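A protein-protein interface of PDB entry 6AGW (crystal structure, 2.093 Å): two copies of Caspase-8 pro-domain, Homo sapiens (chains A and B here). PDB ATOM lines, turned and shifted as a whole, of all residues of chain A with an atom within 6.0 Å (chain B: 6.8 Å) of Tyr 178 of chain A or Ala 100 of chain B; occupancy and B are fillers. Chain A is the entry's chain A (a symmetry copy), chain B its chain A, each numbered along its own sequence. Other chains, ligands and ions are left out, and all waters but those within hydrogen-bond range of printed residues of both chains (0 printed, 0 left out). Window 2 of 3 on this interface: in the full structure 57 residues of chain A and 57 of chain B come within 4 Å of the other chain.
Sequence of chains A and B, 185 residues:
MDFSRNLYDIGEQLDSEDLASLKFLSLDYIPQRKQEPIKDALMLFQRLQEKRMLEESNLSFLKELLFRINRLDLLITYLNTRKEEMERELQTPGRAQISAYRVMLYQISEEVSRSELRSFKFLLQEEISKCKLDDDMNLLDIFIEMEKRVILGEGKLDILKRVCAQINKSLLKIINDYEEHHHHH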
ATOM      1  N   GLU A 154      -5.020 -16.550 -18.128  1.00  0.00           N
ATOM      2  CA  GLU A 154      -3.805 -17.328 -17.908  1.00  0.00           C
ATOM      3  C   GLU A 154      -2.615 -16.820 -18.731  1.00  0.00           C
ATOM      4  O   GLU A 154      -1.468 -16.786 -18.251  1.00  0.00           O
ATOM      5  CB  GLU A 154      -4.072 -18.795 -18.230  1.00  0.00           C
ATOM      6  CG  GLU A 154      -3.313 -19.754 -17.352  1.00  0.00           C
ATOM      7  CD  GLU A 154      -3.907 -21.143 -17.381  1.00  0.00           C
ATOM      8  OE1 GLU A 154      -4.031 -21.705 -18.490  1.00  0.00           O
ATOM      9  OE2 GLU A 154      -4.262 -21.660 -16.299  1.00  0.00           O
ATOM     10  N   GLY A 155      -2.894 -16.442 -19.974  1.00  0.00           N
ATOM     11  CA  GLY A 155      -1.866 -15.914 -20.852  1.00  0.00           C
ATOM     12  C   GLY A 155      -2.078 -14.445 -21.164  1.00  0.00           C
ATOM     13  O   GLY A 155      -1.627 -13.935 -22.197  1.00  0.00           O
ATOM     14  N   LEU A 157      -1.511 -11.517 -18.747  1.00  0.00           N
ATOM     15  CA  LEU A 157      -1.132 -10.922 -17.481  1.00  0.00           C
ATOM     16  C   LEU A 157      -0.549  -9.524 -17.638  1.00  0.00           C
ATOM     17  O   LEU A 157      -0.011  -8.962 -16.683  1.00  0.00           O
ATOM     18  CB  LEU A 157      -0.126 -11.826 -16.772  1.00  0.00           C
ATOM     19  CG  LEU A 157      -0.701 -13.169 -16.326  1.00  0.00           C
ATOM     20  CD1 LEU A 157       0.362 -14.023 -15.679  1.00  0.00           C
ATOM     21  CD2 LEU A 157      -1.855 -12.931 -15.370  1.00  0.00           C
ATOM     22  N   LYS A 173       6.415  -9.488  -8.230  1.00  0.00           N
ATOM     23  CA  LYS A 173       7.191 -10.694  -8.022  1.00  0.00           C
ATOM     24  C   LYS A 173       6.280 -11.909  -7.931  1.00  0.00           C
ATOM     25  O   LYS A 173       6.647 -13.001  -8.393  1.00  0.00           O
ATOM     26  CB  LYS A 173       8.055 -10.594  -6.763  1.00  0.00           C
ATOM     27  CG  LYS A 173       9.371 -11.347  -6.916  1.00  0.00           C
ATOM     28  CD  LYS A 173       9.901 -11.135  -8.342  1.00  0.00           C
ATOM     29  CE  LYS A 173      10.957 -12.147  -8.749  1.00  0.00           C
ATOM     30  NZ  LYS A 173      11.543 -11.767 -10.066  1.00  0.00           N
ATOM     31  N   ILE A 174       5.105 -11.731  -7.324  1.00  0.00           N
ATOM     32  CA  ILE A 174       4.132 -12.819  -7.269  1.00  0.00           C
ATOM     33  C   ILE A 174       3.828 -13.241  -8.702  1.00  0.00           C
ATOM     34  O   ILE A 174       3.962 -14.418  -9.062  1.00  0.00           O
ATOM     35  CB  ILE A 174       2.831 -12.418  -6.528  1.00  0.00           C
ATOM     36  CG1 ILE A 174       3.139 -12.073  -5.072  1.00  0.00           C
ATOM     37  CG2 ILE A 174       1.820 -13.543  -6.584  1.00  0.00           C
ATOM     38  CD1 ILE A 174       1.910 -11.738  -4.234  1.00  0.00           C
ATOM     39  N   ILE A 175       3.489 -12.261  -9.537  1.00  0.00           N
ATOM     40  CA  ILE A 175       3.227 -12.533 -10.947  1.00  0.00           C
ATOM     41  C   ILE A 175       4.400 -13.190 -11.671  1.00  0.00           C
ATOM     42  O   ILE A 175       4.217 -14.190 -12.366  1.00  0.00           O
ATOM     43  CB  ILE A 175       2.848 -11.261 -11.686  1.00  0.00           C
ATOM     44  CG1 ILE A 175       1.631 -10.621 -11.013  1.00  0.00           C
ATOM     45  CG2 ILE A 175       2.563 -11.569 -13.151  1.00  0.00           C
ATOM     46  CD1 ILE A 175       1.248  -9.324 -11.597  1.00  0.00           C
ATOM     47  N   ASN A 176       5.600 -12.644 -11.515  1.00  0.00           N
ATOM     48  CA  ASN A 176       6.754 -13.185 -12.228  1.00  0.00           C
ATOM     49  C   ASN A 176       7.120 -14.599 -11.766  1.00  0.00           C
ATOM     50  O   ASN A 176       7.469 -15.455 -12.583  1.00  0.00           O
ATOM     51  CB  ASN A 176       7.957 -12.252 -12.081  1.00  0.00           C
ATOM     52  CG  ASN A 176       7.852 -11.024 -12.968  1.00  0.00           C
ATOM     53  OD1 ASN A 176       7.260 -11.068 -14.051  1.00  0.00           O
ATOM     54  ND2 ASN A 176       8.428  -9.916 -12.509  1.00  0.00           N
ATOM     55  N   ASP A 177       7.034 -14.842 -10.462  1.00  0.00           N
ATOM     56  CA  ASP A 177       7.301 -16.173  -9.923  1.00  0.00           C
ATOM     57  C   ASP A 177       6.372 -17.209 -10.552  1.00  0.00           C
ATOM     58  O   ASP A 177       6.802 -18.307 -10.909  1.00  0.00           O
ATOM     59  CB  ASP A 177       7.158 -16.186  -8.400  1.00  0.00           C
ATOM     60  CG  ASP A 177       8.351 -15.550  -7.699  1.00  0.00           C
ATOM     61  OD1 ASP A 177       9.314 -15.156  -8.394  1.00  0.00           O
ATOM     62  OD2 ASP A 177       8.329 -15.455  -6.452  1.00  0.00           O
ATOM     63  N   TYR A 178       5.103 -16.842 -10.701  1.00  0.00           N
ATOM     64  CA  TYR A 178       4.137 -17.689 -11.391  1.00  0.00           C
ATOM     65  C   TYR A 178       4.605 -18.038 -12.808  1.00  0.00           C
ATOM     66  O   TYR A 178       4.620 -19.204 -13.191  1.00  0.00           O
ATOM     67  CB  TYR A 178       2.758 -17.005 -11.445  1.00  0.00           C
ATOM     68  CG  TYR A 178       1.837 -17.580 -12.501  1.00  0.00           C
ATOM     69  CD1 TYR A 178       1.213 -18.811 -12.314  1.00  0.00           C
ATOM     70  CD2 TYR A 178       1.609 -16.902 -13.692  1.00  0.00           C
ATOM     71  CE1 TYR A 178       0.384 -19.345 -13.284  1.00  0.00           C
ATOM     72  CE2 TYR A 178       0.782 -17.419 -14.661  1.00  0.00           C
ATOM     73  CZ  TYR A 178       0.172 -18.641 -14.455  1.00  0.00           C
ATOM     74  OH  TYR A 178      -0.651 -19.154 -15.431  1.00  0.00           O
ATOM     75  N   GLU A 179       5.022 -17.039 -13.577  1.00  0.00           N
ATOM     76  CA  GLU A 179       5.139 -17.227 -15.027  1.00  0.00           C
ATOM     77  C   GLU A 179       6.145 -18.276 -15.525  1.00  0.00           C
ATOM     78  O   GLU A 179       6.186 -18.570 -16.719  1.00  0.00           O
ATOM     79  CB  GLU A 179       5.430 -15.887 -15.685  1.00  0.00           C
ATOM     80  CG  GLU A 179       4.332 -15.530 -16.655  1.00  0.00           C
ATOM     81  CD  GLU A 179       4.097 -14.052 -16.748  1.00  0.00           C
ATOM     82  OE1 GLU A 179       4.907 -13.284 -16.188  1.00  0.00           O
ATOM     83  OE2 GLU A 179       3.086 -13.665 -17.369  1.00  0.00           O
ATOM     84  N   GLU A 180       6.928 -18.866 -14.631  1.00  0.00           N
ATOM     85  CA  GLU A 180       7.607 -20.111 -14.987  1.00  0.00           C
ATOM     86  C   GLU A 180       7.698 -21.047 -13.792  1.00  0.00           C
ATOM     87  O   GLU A 180       6.771 -21.817 -13.531  1.00  0.00           O
ATOM     88  CB  GLU A 180       8.995 -19.834 -15.569  1.00  0.00           C
ATOM     89  CG  GLU A 180       9.231 -20.549 -16.897  1.00  0.00           C
ATOM     90  CD  GLU A 180      10.146 -19.783 -17.836  1.00  0.00           C
ATOM     91  OE1 GLU A 180      11.175 -19.253 -17.370  1.00  0.00           O
ATOM     92  OE2 GLU A 180       9.833 -19.718 -19.043  1.00  0.00           O
ATOM     93  N   ARG B  68      -5.447 -23.961   0.143  1.00  0.00           N
ATOM     94  CA  ARG B  68      -5.081 -22.730  -0.547  1.00  0.00           C
ATOM     95  C   ARG B  68      -5.521 -21.462   0.208  1.00  0.00           C
ATOM     96  O   ARG B  68      -4.883 -20.417   0.068  1.00  0.00           O
ATOM     97  CB  ARG B  68      -5.644 -22.720  -1.968  1.00  0.00           C
ATOM     98  CG  ARG B  68      -4.990 -23.735  -2.883  1.00  0.00           C
ATOM     99  CD  ARG B  68      -3.467 -23.607  -2.857  1.00  0.00           C
ATOM    100  NE  ARG B  68      -2.854 -24.360  -3.945  1.00  0.00           N
ATOM    101  CZ  ARG B  68      -1.553 -24.597  -4.052  1.00  0.00           C
ATOM    102  NH1 ARG B  68      -0.715 -24.171  -3.114  1.00  0.00           N
ATOM    103  NH2 ARG B  68      -1.095 -25.280  -5.088  1.00  0.00           N
ATOM    104  N   ALA B  96      -2.987 -30.828  -9.071  1.00  0.00           N
ATOM    105  CA  ALA B  96      -3.756 -29.689  -8.579  1.00  0.00           C
ATOM    106  C   ALA B  96      -4.998 -29.437  -9.434  1.00  0.00           C
ATOM    107  O   ALA B  96      -4.937 -29.353 -10.654  1.00  0.00           O
ATOM    108  CB  ALA B  96      -2.897 -28.449  -8.535  1.00  0.00           C
ATOM    109  N   ILE B  98      -7.063 -26.721  -8.629  1.00  0.00           N
ATOM    110  CA  ILE B  98      -7.169 -25.270  -8.749  1.00  0.00           C
ATOM    111  C   ILE B  98      -5.924 -24.769  -9.462  1.00  0.00           C
ATOM    112  O   ILE B  98      -4.826 -25.053  -9.032  1.00  0.00           O
ATOM    113  CB  ILE B  98      -7.305 -24.579  -7.390  1.00  0.00           C
ATOM    114  CG1 ILE B  98      -8.521 -25.121  -6.636  1.00  0.00           C
ATOM    115  CG2 ILE B  98      -7.441 -23.064  -7.573  1.00  0.00           C
ATOM    116  CD1 ILE B  98      -8.586 -24.684  -5.157  1.00  0.00           C
ATOM    117  N   SER B  99      -6.083 -24.040 -10.557  1.00  0.00           N
ATOM    118  CA  SER B  99      -4.920 -23.691 -11.369  1.00  0.00           C
ATOM    119  C   SER B  99      -4.001 -22.700 -10.657  1.00  0.00           C
ATOM    120  O   SER B  99      -4.458 -21.828  -9.917  1.00  0.00           O
ATOM    121  CB  SER B  99      -5.361 -23.111 -12.714  1.00  0.00           C
ATOM    122  OG  SER B  99      -5.789 -21.769 -12.540  1.00  0.00           O
ATOM    123  N   ALA B 100      -2.703 -22.831 -10.909  1.00  0.00           N
ATOM    124  CA  ALA B 100      -1.710 -21.907 -10.372  1.00  0.00           C
ATOM    125  C   ALA B 100      -2.071 -20.461 -10.726  1.00  0.00           C
ATOM    126  O   ALA B 100      -1.819 -19.559  -9.948  1.00  0.00           O
ATOM    127  CB  ALA B 100      -0.306 -22.260 -10.885  1.00  0.00           C
ATOM    128  N   TYR B 101      -2.715 -20.259 -11.871  1.00  0.00           N
ATOM    129  CA  TYR B 101      -3.191 -18.924 -12.242  1.00  0.00           C
ATOM    130  C   TYR B 101      -4.172 -18.385 -11.192  1.00  0.00           C
ATOM    131  O   TYR B 101      -3.995 -17.285 -10.674  1.00  0.00           O
ATOM    132  CB  TYR B 101      -3.839 -18.961 -13.622  1.00  0.00           C
ATOM    133  CG  TYR B 101      -4.752 -17.784 -13.934  1.00  0.00           C
ATOM    134  CD1 TYR B 101      -4.230 -16.532 -14.260  1.00  0.00           C
ATOM    135  CD2 TYR B 101      -6.140 -17.934 -13.918  1.00  0.00           C
ATOM    136  CE1 TYR B 101      -5.062 -15.458 -14.564  1.00  0.00           C
ATOM    137  CE2 TYR B 101      -6.988 -16.869 -14.218  1.00  0.00           C
ATOM    138  CZ  TYR B 101      -6.439 -15.635 -14.546  1.00  0.00           C
ATOM    139  OH  TYR B 101      -7.266 -14.579 -14.837  1.00  0.00           O
ATOM    140  N   ARG B 102      -5.182 -19.186 -10.858  1.00  0.00           N
ATOM    141  CA  ARG B 102      -6.205 -18.796  -9.887  1.00  0.00           C
ATOM    142  C   ARG B 102      -5.578 -18.541  -8.512  1.00  0.00           C
ATOM    143  O   ARG B 102      -5.870 -17.549  -7.843  1.00  0.00           O
ATOM    144  CB  ARG B 102      -7.284 -19.885  -9.812  1.00  0.00           C
ATOM    145  CG  ARG B 102      -8.566 -19.501  -9.106  1.00  0.00           C
ATOM    146  CD  ARG B 102      -9.296 -18.399  -9.836  1.00  0.00           C
ATOM    147  NE  ARG B 102      -9.813 -18.806 -11.142  1.00  0.00           N
ATOM    148  CZ  ARG B 102     -10.401 -17.963 -11.983  1.00  0.00           C
ATOM    149  NH1 ARG B 102     -10.545 -16.689 -11.636  1.00  0.00           N
ATOM    150  NH2 ARG B 102     -10.840 -18.382 -13.161  1.00  0.00           N
ATOM    151  N   VAL B 103      -4.678 -19.422  -8.107  1.00  0.00           N
ATOM    152  CA  VAL B 103      -4.000 -19.270  -6.828  1.00  0.00           C
ATOM    153  C   VAL B 103      -3.179 -17.974  -6.791  1.00  0.00           C
ATOM    154  O   VAL B 103      -3.190 -17.231  -5.797  1.00  0.00           O
ATOM    155  CB  VAL B 103      -3.091 -20.494  -6.542  1.00  0.00           C
ATOM    156  CG1 VAL B 103      -2.110 -20.201  -5.419  1.00  0.00           C
ATOM    157  CG2 VAL B 103      -3.943 -21.717  -6.218  1.00  0.00           C
ATOM    158  N   MET B 104      -2.480 -17.705  -7.891  1.00  0.00           N
ATOM    159  CA  MET B 104      -1.694 -16.485  -8.035  1.00  0.00           C
ATOM    160  C   MET B 104      -2.540 -15.216  -7.804  1.00  0.00           C
ATOM    161  O   MET B 104      -2.150 -14.332  -7.040  1.00  0.00           O
ATOM    162  CB  MET B 104      -1.046 -16.456  -9.419  1.00  0.00           C
ATOM    163  CG  MET B 104      -0.084 -15.310  -9.645  1.00  0.00           C
ATOM    164  SD  MET B 104      -0.854 -13.853 -10.355  1.00  0.00           S
ATOM    165  CE  MET B 104      -1.513 -14.461 -11.918  1.00  0.00           C
ATOM    166  N   LEU B 105      -3.698 -15.115  -8.446  1.00  0.00           N
ATOM    167  CA  LEU B 105      -4.539 -13.928  -8.230  1.00  0.00           C
ATOM    168  C   LEU B 105      -5.001 -13.851  -6.777  1.00  0.00           C
ATOM    169  O   LEU B 105      -5.039 -12.769  -6.175  1.00  0.00           O
ATOM    170  CB  LEU B 105      -5.737 -13.934  -9.169  1.00  0.00           C
ATOM    171  CG  LEU B 105      -5.404 -13.942 -10.666  1.00  0.00           C
ATOM    172  CD1 LEU B 105      -6.663 -14.138 -11.498  1.00  0.00           C
ATOM    173  CD2 LEU B 105      -4.678 -12.675 -11.067  1.00  0.00           C
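No position is printed for both chains.
The side-chain hydroxyl (OG) of Ser 99 of chain B sits close to the backbone NH (N) of Tyr 101 of chain B (3.5 Å).
Printed residues of chain A that touch a printed residue of chain B: Glu 154, Leu 157 and Tyr 178.
Hydrophobic or aromatic side chains of chain A that line the printed part of chain B: Leu 157 and Tyr 178.
Hydrophobic or aromatic side chains of chain B that line the printed part of chain A: Ala 100, Tyr 101 and Met 104.
Among the printed residues, no Asp or Glu carboxylate lies within 4 Å of a Lys or Arg side-chain nitrogen of the other chain.
Tyr 101 of chain B touches Glu 154 of chain A.
Met 104 of chain B touches Leu 157 of chain A (CE to CD2, 3.8 Å).
Ala 100 of chain B touches Tyr 178 of chain A.
Tyr 178 of chain A touches Tyr 101 of chain B (CE1 to N, 3.5 Å).
Tyr 178 of chain A touches Met 104 of chain B.
Of chain B, only Ala 100 (3.7 Å), Tyr 101 (3.5 Å) and Met 104 (3.8 Å) come within 4 Å of Tyr 178 of chain A.
Printed residues of chain B within 4 Å of Leu 157 of chain A: Met 104 (3.8 Å).
Of the printed residues of chain B, Glu 154 of chain A touches Tyr 101 (3.7 Å).
Printed residues of chain A within 4 Å of Met 104 of chain B: Leu 157 and Tyr 178.
Of the printed residues of chain A, Tyr 101 of chain B touches Glu 154 (3.7 Å) and Tyr 178 (3.5 Å).
Glu 179 of chain A touches none of the printed residues of chain B.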
